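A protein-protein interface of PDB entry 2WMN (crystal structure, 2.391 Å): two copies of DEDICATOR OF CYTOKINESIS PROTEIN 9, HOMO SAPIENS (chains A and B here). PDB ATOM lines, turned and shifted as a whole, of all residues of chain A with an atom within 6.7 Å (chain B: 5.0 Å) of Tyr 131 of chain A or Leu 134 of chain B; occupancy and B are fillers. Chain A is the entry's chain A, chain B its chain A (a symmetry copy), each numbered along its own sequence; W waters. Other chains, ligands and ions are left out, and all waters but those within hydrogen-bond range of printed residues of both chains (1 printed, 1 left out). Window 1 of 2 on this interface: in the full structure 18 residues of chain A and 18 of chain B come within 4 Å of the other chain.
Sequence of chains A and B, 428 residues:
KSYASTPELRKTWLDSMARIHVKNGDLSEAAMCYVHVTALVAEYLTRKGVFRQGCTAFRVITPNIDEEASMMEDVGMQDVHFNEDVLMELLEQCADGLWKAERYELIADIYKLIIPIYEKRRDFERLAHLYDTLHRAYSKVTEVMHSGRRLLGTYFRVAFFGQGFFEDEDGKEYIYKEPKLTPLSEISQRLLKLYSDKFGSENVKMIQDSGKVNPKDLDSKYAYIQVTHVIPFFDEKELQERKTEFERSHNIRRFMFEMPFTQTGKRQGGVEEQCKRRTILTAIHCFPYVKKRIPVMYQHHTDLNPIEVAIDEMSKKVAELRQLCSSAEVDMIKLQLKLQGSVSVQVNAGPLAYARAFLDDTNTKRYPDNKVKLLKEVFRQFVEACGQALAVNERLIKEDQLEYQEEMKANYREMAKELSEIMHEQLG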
ATOM      1  N   TYR A 111     -10.513  16.729  12.654  1.00  0.00           N
ATOM      2  CA  TYR A 111     -10.897  17.224  11.343  1.00  0.00           C
ATOM      3  C   TYR A 111     -11.981  18.280  11.416  1.00  0.00           C
ATOM      4  O   TYR A 111     -11.997  19.203  10.616  1.00  0.00           O
ATOM      5  CB  TYR A 111     -11.290  16.080  10.444  1.00  0.00           C
ATOM      6  CG  TYR A 111     -10.107  15.518   9.713  1.00  0.00           C
ATOM      7  CD1 TYR A 111      -9.025  16.333   9.378  1.00  0.00           C
ATOM      8  CD2 TYR A 111     -10.070  14.193   9.329  1.00  0.00           C
ATOM      9  CE1 TYR A 111      -7.944  15.832   8.671  1.00  0.00           C
ATOM     10  CE2 TYR A 111      -8.982  13.686   8.641  1.00  0.00           C
ATOM     11  CZ  TYR A 111      -7.940  14.511   8.311  1.00  0.00           C
ATOM     12  OH  TYR A 111      -6.884  14.003   7.618  1.00  0.00           O
ATOM     13  N   ILE A 115     -12.045  21.489   8.856  1.00  0.00           N
ATOM     14  CA  ILE A 115     -13.058  21.492   7.815  1.00  0.00           C
ATOM     15  C   ILE A 115     -13.475  22.929   7.421  1.00  0.00           C
ATOM     16  O   ILE A 115     -13.426  23.299   6.256  1.00  0.00           O
ATOM     17  CB  ILE A 115     -14.256  20.547   8.186  1.00  0.00           C
ATOM     18  CG1 ILE A 115     -13.857  19.090   7.972  1.00  0.00           C
ATOM     19  CG2 ILE A 115     -15.517  20.829   7.329  1.00  0.00           C
ATOM     20  CD1 ILE A 115     -14.853  18.088   8.464  1.00  0.00           C
ATOM     21  N   GLU A 119     -13.086  24.684   3.810  1.00  0.00           N
ATOM     22  CA  GLU A 119     -14.266  25.199   3.090  1.00  0.00           C
ATOM     23  C   GLU A 119     -14.065  26.639   2.681  1.00  0.00           C
ATOM     24  O   GLU A 119     -14.287  27.002   1.535  1.00  0.00           O
ATOM     25  CB  GLU A 119     -15.552  25.037   3.911  1.00  0.00           C
ATOM     26  CG  GLU A 119     -15.935  23.569   4.086  1.00  0.00           C
ATOM     27  CD  GLU A 119     -17.000  23.343   5.117  1.00  0.00           C
ATOM     28  OE1 GLU A 119     -17.190  24.222   5.983  1.00  0.00           O
ATOM     29  OE2 GLU A 119     -17.662  22.277   5.071  1.00  0.00           O
ATOM     30  N   ARG A 126      -8.598  18.558  -0.606  1.00  0.00           N
ATOM     31  CA  ARG A 126      -8.345  18.315   0.814  1.00  0.00           C
ATOM     32  C   ARG A 126      -9.571  17.781   1.521  1.00  0.00           C
ATOM     33  O   ARG A 126      -9.466  16.881   2.362  1.00  0.00           O
ATOM     34  CB  ARG A 126      -7.926  19.602   1.531  1.00  0.00           C
ATOM     35  CG  ARG A 126      -6.573  20.192   1.146  1.00  0.00           C
ATOM     36  CD  ARG A 126      -5.455  19.176   1.086  1.00  0.00           C
ATOM     37  NE  ARG A 126      -4.163  19.759   1.460  1.00  0.00           N
ATOM     38  CZ  ARG A 126      -3.476  20.651   0.733  1.00  0.00           C
ATOM     39  NH1 ARG A 126      -3.962  21.124  -0.422  1.00  0.00           N
ATOM     40  NH2 ARG A 126      -2.297  21.094   1.176  1.00  0.00           N
ATOM     41  N   LEU A 127     -10.734  18.354   1.202  1.00  0.00           N
ATOM     42  CA  LEU A 127     -11.972  17.943   1.873  1.00  0.00           C
ATOM     43  C   LEU A 127     -12.274  16.518   1.483  1.00  0.00           C
ATOM     44  O   LEU A 127     -12.687  15.721   2.313  1.00  0.00           O
ATOM     45  CB  LEU A 127     -13.149  18.868   1.541  1.00  0.00           C
ATOM     46  CG  LEU A 127     -13.056  20.253   2.171  1.00  0.00           C
ATOM     47  CD1 LEU A 127     -13.857  21.227   1.363  1.00  0.00           C
ATOM     48  CD2 LEU A 127     -13.476  20.281   3.636  1.00  0.00           C
ATOM     49  N   ALA A 128     -12.044  16.196   0.214  1.00  0.00           N
ATOM     50  CA  ALA A 128     -12.281  14.841  -0.286  1.00  0.00           C
ATOM     51  C   ALA A 128     -11.445  13.846   0.509  1.00  0.00           C
ATOM     52  O   ALA A 128     -11.931  12.801   0.937  1.00  0.00           O
ATOM     53  CB  ALA A 128     -11.937  14.751  -1.787  1.00  0.00           C
ATOM     54  N   HIS A 129     -10.180  14.196   0.693  1.00  0.00           N
ATOM     55  CA  HIS A 129      -9.230  13.346   1.384  1.00  0.00           C
ATOM     56  C   HIS A 129      -9.626  13.145   2.835  1.00  0.00           C
ATOM     57  O   HIS A 129      -9.754  12.006   3.308  1.00  0.00           O
ATOM     58  CB  HIS A 129      -7.828  13.941   1.311  1.00  0.00           C
ATOM     59  CG  HIS A 129      -6.805  13.105   2.014  1.00  0.00           C
ATOM     60  ND1 HIS A 129      -6.122  13.539   3.134  1.00  0.00           N
ATOM     61  CD2 HIS A 129      -6.387  11.836   1.785  1.00  0.00           C
ATOM     62  CE1 HIS A 129      -5.308  12.581   3.544  1.00  0.00           C
ATOM     63  NE2 HIS A 129      -5.450  11.539   2.741  1.00  0.00           N
ATOM     64  N   LEU A 130      -9.870  14.248   3.536  1.00  0.00           N
ATOM     65  CA  LEU A 130     -10.250  14.103   4.928  1.00  0.00           C
ATOM     66  C   LEU A 130     -11.492  13.236   5.099  1.00  0.00           C
ATOM     67  O   LEU A 130     -11.506  12.351   5.963  1.00  0.00           O
ATOM     68  CB  LEU A 130     -10.348  15.452   5.641  1.00  0.00           C
ATOM     69  CG  LEU A 130     -11.520  16.403   5.543  1.00  0.00           C
ATOM     70  CD1 LEU A 130     -12.744  15.896   6.347  1.00  0.00           C
ATOM     71  CD2 LEU A 130     -11.035  17.740   6.055  1.00  0.00           C
ATOM     72  N   TYR A 131     -12.509  13.442   4.259  1.00  0.00           N
ATOM     73  CA  TYR A 131     -13.731  12.631   4.362  1.00  0.00           C
ATOM     74  C   TYR A 131     -13.511  11.183   3.904  1.00  0.00           C
ATOM     75  O   TYR A 131     -14.212  10.265   4.347  1.00  0.00           O
ATOM     76  CB  TYR A 131     -14.901  13.266   3.574  1.00  0.00           C
ATOM     77  CG  TYR A 131     -15.420  14.584   4.124  1.00  0.00           C
ATOM     78  CD1 TYR A 131     -15.917  14.670   5.413  1.00  0.00           C
ATOM     79  CD2 TYR A 131     -15.423  15.733   3.341  1.00  0.00           C
ATOM     80  CE1 TYR A 131     -16.396  15.850   5.911  1.00  0.00           C
ATOM     81  CE2 TYR A 131     -15.894  16.938   3.841  1.00  0.00           C
ATOM     82  CZ  TYR A 131     -16.393  16.980   5.116  1.00  0.00           C
ATOM     83  OH  TYR A 131     -16.884  18.158   5.627  1.00  0.00           O
ATOM     84  N   ASP A 132     -12.552  10.976   3.004  1.00  0.00           N
ATOM     85  CA  ASP A 132     -12.128   9.611   2.705  1.00  0.00           C
ATOM     86  C   ASP A 132     -11.556   8.935   3.979  1.00  0.00           C
ATOM     87  O   ASP A 132     -11.947   7.827   4.345  1.00  0.00           O
ATOM     88  CB  ASP A 132     -11.093   9.585   1.583  1.00  0.00           C
ATOM     89  CG  ASP A 132     -10.760   8.161   1.143  1.00  0.00           C
ATOM     90  OD1 ASP A 132     -11.635   7.279   1.277  1.00  0.00           O
ATOM     91  OD2 ASP A 132      -9.627   7.919   0.669  1.00  0.00           O
ATOM     92  N   THR A 133     -10.664   9.632   4.671  1.00  0.00           N
ATOM     93  CA  THR A 133     -10.130   9.115   5.913  1.00  0.00           C
ATOM     94  C   THR A 133     -11.213   8.828   6.946  1.00  0.00           C
ATOM     95  O   THR A 133     -11.191   7.772   7.592  1.00  0.00           O
ATOM     96  CB  THR A 133      -9.109  10.074   6.504  1.00  0.00           C
ATOM     97  OG1 THR A 133      -8.003  10.176   5.611  1.00  0.00           O
ATOM     98  CG2 THR A 133      -8.625   9.570   7.835  1.00  0.00           C
ATOM     99  N   LEU A 134     -12.164   9.748   7.115  1.00  0.00           N
ATOM    100  CA  LEU A 134     -13.256   9.523   8.083  1.00  0.00           C
ATOM    101  C   LEU A 134     -14.129   8.340   7.710  1.00  0.00           C
ATOM    102  O   LEU A 134     -14.638   7.612   8.562  1.00  0.00           O
ATOM    103  CB  LEU A 134     -14.136  10.759   8.234  1.00  0.00           C
ATOM    104  CG  LEU A 134     -13.412  11.918   8.902  1.00  0.00           C
ATOM    105  CD1 LEU A 134     -14.310  13.192   8.973  1.00  0.00           C
ATOM    106  CD2 LEU A 134     -12.871  11.466  10.306  1.00  0.00           C
ATOM    107  N   HIS A 135     -14.306   8.131   6.419  1.00  0.00           N
ATOM    108  CA  HIS A 135     -15.122   7.012   6.007  1.00  0.00           C
ATOM    109  C   HIS A 135     -14.397   5.704   6.351  1.00  0.00           C
ATOM    110  O   HIS A 135     -14.956   4.800   6.960  1.00  0.00           O
ATOM    111  CB  HIS A 135     -15.389   7.097   4.511  1.00  0.00           C
ATOM    112  CG  HIS A 135     -15.836   5.801   3.916  1.00  0.00           C
ATOM    113  ND1 HIS A 135     -17.001   5.181   4.301  1.00  0.00           N
ATOM    114  CD2 HIS A 135     -15.261   5.004   2.988  1.00  0.00           C
ATOM    115  CE1 HIS A 135     -17.138   4.052   3.618  1.00  0.00           C
ATOM    116  NE2 HIS A 135     -16.096   3.929   2.814  1.00  0.00           N
ATOM    117  N   ARG A 136     -13.150   5.605   5.927  1.00  0.00           N
ATOM    118  CA  ARG A 136     -12.347   4.468   6.288  1.00  0.00           C
ATOM    119  C   ARG A 136     -12.330   4.300   7.813  1.00  0.00           C
ATOM    120  O   ARG A 136     -12.605   3.212   8.326  1.00  0.00           O
ATOM    121  CB  ARG A 136     -10.939   4.677   5.764  1.00  0.00           C
ATOM    122  CG  ARG A 136     -10.833   4.626   4.252  1.00  0.00           C
ATOM    123  CD  ARG A 136      -9.475   5.231   3.854  1.00  0.00           C
ATOM    124  NE  ARG A 136      -9.059   4.995   2.473  1.00  0.00           N
ATOM    125  CZ  ARG A 136      -9.545   4.054   1.659  1.00  0.00           C
ATOM    126  NH1 ARG A 136     -10.492   3.211   2.057  1.00  0.00           N
ATOM    127  NH2 ARG A 136      -9.068   3.956   0.424  1.00  0.00           N
ATOM    128  N   ILE B 107     -24.127  19.434   0.419  1.00  0.00           N
ATOM    129  CA  ILE B 107     -24.433  18.280   1.266  1.00  0.00           C
ATOM    130  C   ILE B 107     -23.854  18.360   2.684  1.00  0.00           C
ATOM    131  O   ILE B 107     -24.487  17.913   3.655  1.00  0.00           O
ATOM    132  CB  ILE B 107     -23.991  16.964   0.621  1.00  0.00           C
ATOM    133  CG1 ILE B 107     -24.705  16.812  -0.736  1.00  0.00           C
ATOM    134  CG2 ILE B 107     -24.324  15.815   1.571  1.00  0.00           C
ATOM    135  CD1 ILE B 107     -24.197  15.694  -1.620  1.00  0.00           C
ATOM    136  N   ALA B 108     -22.655  18.932   2.804  1.00  0.00           N
ATOM    137  CA  ALA B 108     -21.998  19.014   4.113  1.00  0.00           C
ATOM    138  C   ALA B 108     -22.817  19.878   5.079  1.00  0.00           C
ATOM    139  O   ALA B 108     -22.866  19.611   6.275  1.00  0.00           O
ATOM    140  CB  ALA B 108     -20.540  19.521   3.987  1.00  0.00           C
ATOM    141  N   TYR B 111     -25.309  17.459   6.570  1.00  0.00           N
ATOM    142  CA  TYR B 111     -24.751  16.397   7.390  1.00  0.00           C
ATOM    143  C   TYR B 111     -24.151  16.915   8.681  1.00  0.00           C
ATOM    144  O   TYR B 111     -24.213  16.247   9.701  1.00  0.00           O
ATOM    145  CB  TYR B 111     -23.759  15.586   6.597  1.00  0.00           C
ATOM    146  CG  TYR B 111     -24.423  14.458   5.863  1.00  0.00           C
ATOM    147  CD1 TYR B 111     -25.569  13.852   6.379  1.00  0.00           C
ATOM    148  CD2 TYR B 111     -23.905  13.974   4.680  1.00  0.00           C
ATOM    149  CE1 TYR B 111     -26.170  12.787   5.728  1.00  0.00           C
ATOM    150  CE2 TYR B 111     -24.515  12.924   4.018  1.00  0.00           C
ATOM    151  CZ  TYR B 111     -25.629  12.336   4.554  1.00  0.00           C
ATOM    152  OH  TYR B 111     -26.209  11.292   3.902  1.00  0.00           O
ATOM    153  N   LYS B 112     -23.634  18.137   8.647  1.00  0.00           N
ATOM    154  CA  LYS B 112     -23.061  18.729   9.841  1.00  0.00           C
ATOM    155  C   LYS B 112     -24.120  18.727  10.906  1.00  0.00           C
ATOM    156  O   LYS B 112     -23.788  18.683  12.073  1.00  0.00           O
ATOM    157  CB  LYS B 112     -22.648  20.181   9.609  1.00  0.00           C
ATOM    158  CG  LYS B 112     -21.304  20.398   8.963  1.00  0.00           C
ATOM    159  CD  LYS B 112     -21.201  21.881   8.482  1.00  0.00           C
ATOM    160  CE  LYS B 112     -19.771  22.223   8.009  1.00  0.00           C
ATOM    161  NZ  LYS B 112     -19.201  21.236   7.052  1.00  0.00           N
ATOM    162  N   ILE B 115     -24.423  14.801  12.190  1.00  0.00           N
ATOM    163  CA  ILE B 115     -23.215  14.161  12.678  1.00  0.00           C
ATOM    164  C   ILE B 115     -23.205  14.051  14.222  1.00  0.00           C
ATOM    165  O   ILE B 115     -23.036  12.971  14.772  1.00  0.00           O
ATOM    166  CB  ILE B 115     -21.932  14.829  12.067  1.00  0.00           C
ATOM    167  CG1 ILE B 115     -21.743  14.373  10.624  1.00  0.00           C
ATOM    168  CG2 ILE B 115     -20.646  14.467  12.856  1.00  0.00           C
ATOM    169  CD1 ILE B 115     -20.658  15.082   9.878  1.00  0.00           C
ATOM    170  N   LEU B 130     -22.433   8.472   5.753  1.00  0.00           N
ATOM    171  CA  LEU B 130     -22.445   9.893   5.467  1.00  0.00           C
ATOM    172  C   LEU B 130     -21.091  10.394   4.979  1.00  0.00           C
ATOM    173  O   LEU B 130     -21.032  11.136   3.991  1.00  0.00           O
ATOM    174  CB  LEU B 130     -23.012  10.709   6.629  1.00  0.00           C
ATOM    175  CG  LEU B 130     -22.247  11.087   7.879  1.00  0.00           C
ATOM    176  CD1 LEU B 130     -21.211  12.206   7.606  1.00  0.00           C
ATOM    177  CD2 LEU B 130     -23.275  11.519   8.900  1.00  0.00           C
ATOM    178  N   TYR B 131     -20.004   9.961   5.622  1.00  0.00           N
ATOM    179  CA  TYR B 131     -18.666  10.396   5.194  1.00  0.00           C
ATOM    180  C   TYR B 131     -18.250   9.771   3.855  1.00  0.00           C
ATOM    181  O   TYR B 131     -17.443  10.343   3.112  1.00  0.00           O
ATOM    182  CB  TYR B 131     -17.600  10.098   6.274  1.00  0.00           C
ATOM    183  CG  TYR B 131     -17.731  10.899   7.559  1.00  0.00           C
ATOM    184  CD1 TYR B 131     -17.685  12.282   7.543  1.00  0.00           C
ATOM    185  CD2 TYR B 131     -17.885  10.261   8.785  1.00  0.00           C
ATOM    186  CE1 TYR B 131     -17.791  13.008   8.697  1.00  0.00           C
ATOM    187  CE2 TYR B 131     -18.007  10.989   9.959  1.00  0.00           C
ATOM    188  CZ  TYR B 131     -17.940  12.356   9.905  1.00  0.00           C
ATOM    189  OH  TYR B 131     -18.039  13.098  11.058  1.00  0.00           O
ATOM    190  N   ASP B 132     -18.783   8.589   3.553  1.00  0.00           N
ATOM    191  CA  ASP B 132     -18.623   8.051   2.204  1.00  0.00           C
ATOM    192  C   ASP B 132     -19.279   9.001   1.167  1.00  0.00           C
ATOM    193  O   ASP B 132     -18.664   9.382   0.170  1.00  0.00           O
ATOM    194  CB  ASP B 132     -19.220   6.651   2.090  1.00  0.00           C
ATOM    195  CG  ASP B 132     -18.919   6.007   0.739  1.00  0.00           C
ATOM    196  OD1 ASP B 132     -17.878   6.350   0.138  1.00  0.00           O
ATOM    197  OD2 ASP B 132     -19.719   5.165   0.273  1.00  0.00           O
ATOM    198  N   THR B 133     -20.511   9.413   1.435  1.00  0.00           N
ATOM    199  CA  THR B 133     -21.177  10.358   0.564  1.00  0.00           C
ATOM    200  C   THR B 133     -20.407  11.665   0.414  1.00  0.00           C
ATOM    201  O   THR B 133     -20.261  12.176  -0.704  1.00  0.00           O
ATOM    202  CB  THR B 133     -22.582  10.654   1.061  1.00  0.00           C
ATOM    203  OG1 THR B 133     -23.352   9.456   1.003  1.00  0.00           O
ATOM    204  CG2 THR B 133     -23.234  11.701   0.200  1.00  0.00           C
ATOM    205  N   LEU B 134     -19.907  12.217   1.521  1.00  0.00           N
ATOM    206  CA  LEU B 134     -19.132  13.471   1.444  1.00  0.00           C
ATOM    207  C   LEU B 134     -17.846  13.311   0.655  1.00  0.00           C
ATOM    208  O   LEU B 134     -17.393  14.220  -0.042  1.00  0.00           O
ATOM    209  CB  LEU B 134     -18.796  14.010   2.830  1.00  0.00           C
ATOM    210  CG  LEU B 134     -20.025  14.494   3.586  1.00  0.00           C
ATOM    211  CD1 LEU B 134     -19.662  14.967   5.029  1.00  0.00           C
ATOM    212  CD2 LEU B 134     -20.764  15.595   2.744  1.00  0.00           C
ATOM    213  N   HIS B 135     -17.246  12.141   0.750  1.00  0.00           N
ATOM    214  CA  HIS B 135     -16.022  11.930   0.010  1.00  0.00           C
ATOM    215  C   HIS B 135     -16.337  11.902  -1.491  1.00  0.00           C
ATOM    216  O   HIS B 135     -15.710  12.584  -2.292  1.00  0.00           O
ATOM    217  CB  HIS B 135     -15.379  10.621   0.446  1.00  0.00           C
ATOM    218  CG  HIS B 135     -14.375  10.102  -0.532  1.00  0.00           C
ATOM    219  ND1 HIS B 135     -13.234  10.800  -0.850  1.00  0.00           N
ATOM    220  CD2 HIS B 135     -14.358   8.973  -1.273  1.00  0.00           C
ATOM    221  CE1 HIS B 135     -12.538  10.109  -1.743  1.00  0.00           C
ATOM    222  NE2 HIS B 135     -13.201   8.996  -2.010  1.00  0.00           N
ATOM    223  N   ARG B 136     -17.301  11.081  -1.865  1.00  0.00           N
ATOM    224  CA  ARG B 136     -17.748  11.057  -3.231  1.00  0.00           C
ATOM    225  C   ARG B 136     -18.147  12.470  -3.678  1.00  0.00           C
ATOM    226  O   ARG B 136     -17.685  12.952  -4.716  1.00  0.00           O
ATOM    227  CB  ARG B 136     -18.931  10.114  -3.343  1.00  0.00           C
ATOM    228  CG  ARG B 136     -18.573   8.654  -3.140  1.00  0.00           C
ATOM    229  CD  ARG B 136     -19.879   7.880  -2.889  1.00  0.00           C
ATOM    230  NE  ARG B 136     -19.775   6.424  -2.973  1.00  0.00           N
ATOM    231  CZ  ARG B 136     -18.792   5.742  -3.565  1.00  0.00           C
ATOM    232  NH1 ARG B 136     -17.776   6.360  -4.158  1.00  0.00           N
ATOM    233  NH2 ARG B 136     -18.831   4.415  -3.565  1.00  0.00           N
ATOM    234  N   ALA B 137     -18.983  13.144  -2.885  1.00  0.00           N
ATOM    235  CA  ALA B 137     -19.446  14.480  -3.278  1.00  0.00           C
ATOM    236  C   ALA B 137     -18.277  15.389  -3.621  1.00  0.00           C
ATOM    237  O   ALA B 137     -18.261  16.007  -4.697  1.00  0.00           O
ATOM    238  CB  ALA B 137     -20.339  15.105  -2.211  1.00  0.00           C
ATOM    239  N   TYR B 138     -17.285  15.467  -2.733  1.00  0.00           N
ATOM    240  CA  TYR B 138     -16.166  16.395  -2.972  1.00  0.00           C
ATOM    241  C   TYR B 138     -15.279  15.891  -4.093  1.00  0.00           C
ATOM    242  O   TYR B 138     -14.542  16.646  -4.729  1.00  0.00           O
ATOM    243  CB  TYR B 138     -15.376  16.719  -1.685  1.00  0.00           C
ATOM    244  CG  TYR B 138     -16.137  17.698  -0.819  1.00  0.00           C
ATOM    245  CD1 TYR B 138     -16.132  19.057  -1.108  1.00  0.00           C
ATOM    246  CD2 TYR B 138     -16.903  17.259   0.240  1.00  0.00           C
ATOM    247  CE1 TYR B 138     -16.854  19.944  -0.367  1.00  0.00           C
ATOM    248  CE2 TYR B 138     -17.614  18.143   1.008  1.00  0.00           C
ATOM    249  CZ  TYR B 138     -17.593  19.491   0.694  1.00  0.00           C
ATOM    250  OH  TYR B 138     -18.316  20.398   1.454  1.00  0.00           O
ATOM    251  N   SER B 139     -15.393  14.598  -4.350  1.00  0.00           N
ATOM    252  CA  SER B 139     -14.728  13.992  -5.488  1.00  0.00           C
ATOM    253  C   SER B 139     -15.405  14.438  -6.798  1.00  0.00           C
ATOM    254  O   SER B 139     -14.736  14.902  -7.716  1.00  0.00           O
ATOM    255  CB  SER B 139     -14.761  12.476  -5.348  1.00  0.00           C
ATOM    256  OG  SER B 139     -13.471  11.983  -5.606  1.00  0.00           O
HETATM  257  O   HOH W   1     -18.592  18.761   7.853  1.00  0.00           O
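The backbone carbonyl oxygen (O) of Tyr 131 of chain B lies close to the backbone carbonyl oxygen (O) of Tyr 131 of chain A (3.5 Å). The side-chain amino group (NZ) of Lys 112 of chain B is in salt-bridge range of the side-chain carboxylate (OE2) of Glu 119 of chain A (2.7 Å). O of Ala 128 of chain A is in hydrogen-bond range of ND1 of His 135 of chain B (3.0 Å).
NE of Arg 136 of chain A lies within salt-bridge range of OD2 of Asp 132 of chain A. The guanidinium group of Arg 136 of chain B is in salt-bridge range of the side-chain carboxylate of Asp 132 of chain B, 3.5 Å away.
Among the printed residues, pairs that only touch across the chains: Ile 115 of chain A with Lys 112 of chain B (3.7 Å), Leu 127 of chain A with Tyr 138 of chain B (3.7 Å), Ala 128 of chain A with Tyr 138 of chain B (3.9 Å), Tyr 131 of chain A with Leu 134 of chain B (3.5 Å), Tyr 131 of chain A with His 135 of chain B (3.8 Å), Tyr 131 of chain A with Tyr 138 of chain B (3.5 Å), Asp 132 of chain A with His 135 of chain B (3.5 Å), Leu 134 of chain A with Tyr 131 of chain B (3.5 Å), His 135 of chain A with Tyr 131 of chain B (3.8 Å) and His 135 of chain A with Asp 132 of chain B (3.5 Å).
Of chain B, only Tyr 131, Leu 134, His 135 and Tyr 138 come within 4 Å of Tyr 131 of chain A. Leu 134 of chain B touches just one residue of chain A: Tyr 131. Of the printed residues of chain B, Glu 119 of chain A touches Lys 112 (2.7 Å). Of the printed residues of chain A, Lys 112 of chain B touches Ile 115 and Glu 119. Of the printed residues of chain A, Tyr 138 of chain B touches Leu 127, Ala 128 and Tyr 131. Of the printed residues of chain B, His 135 of chain A touches Tyr 131 and Asp 132. Thr 133 of chain A touches none of the printed residues of chain B. Ser 139 of chain B touches none of the printed residues of chain A. The nearest residue of chain A that does not touch Leu 134 of chain B is Ala 128 of chain A (5.2 Å).
Printed residues of chain A that touch a printed residue of chain B: Ile 115, Glu 119, Leu 127, Ala 128, Tyr 131, Asp 132, Leu 134 and His 135. Hydrophobic or aromatic side chains of chain A that line the printed part of chain B: Ile 115, Leu 127, Ala 128, Tyr 131, Leu 134 and His 135. Of the 15 printed residues of chain B, 6 touch a printed residue of chain A. Printed residues of chain B that touch a printed residue of chain A: Lys 112, Tyr 131, Asp 132, Leu 134, His 135 and Tyr 138. Hydrophobic or aromatic side chains of chain B that line the printed part of chain A: Tyr 131, Leu 134, His 135 and Tyr 138. Among the printed residues, 13 pairs touch across the chains.
Tyr 131 of chain A touches its own counterpart, Tyr 131 of chain B. Tyr 131 of chain A touches Leu 134 of chain B, and with the chains exchanged Leu 134 of chain A touches Tyr 131 of chain B. Tyr 131 of chain A touches His 135 of chain B, and with the chains exchanged His 135 of chain A touches Tyr 131 of chain B. Asp 132 of chain A touches His 135 of chain B, and with the chains exchanged His 135 of chain A touches Asp 132 of chain B. Positions printed for both chains: 111, 115, 130, 131, 132, 133, 134, 135 and 136.
Water W1 bridges NZ of Lys 112 of chain B and OH of Tyr 131 of chain A.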
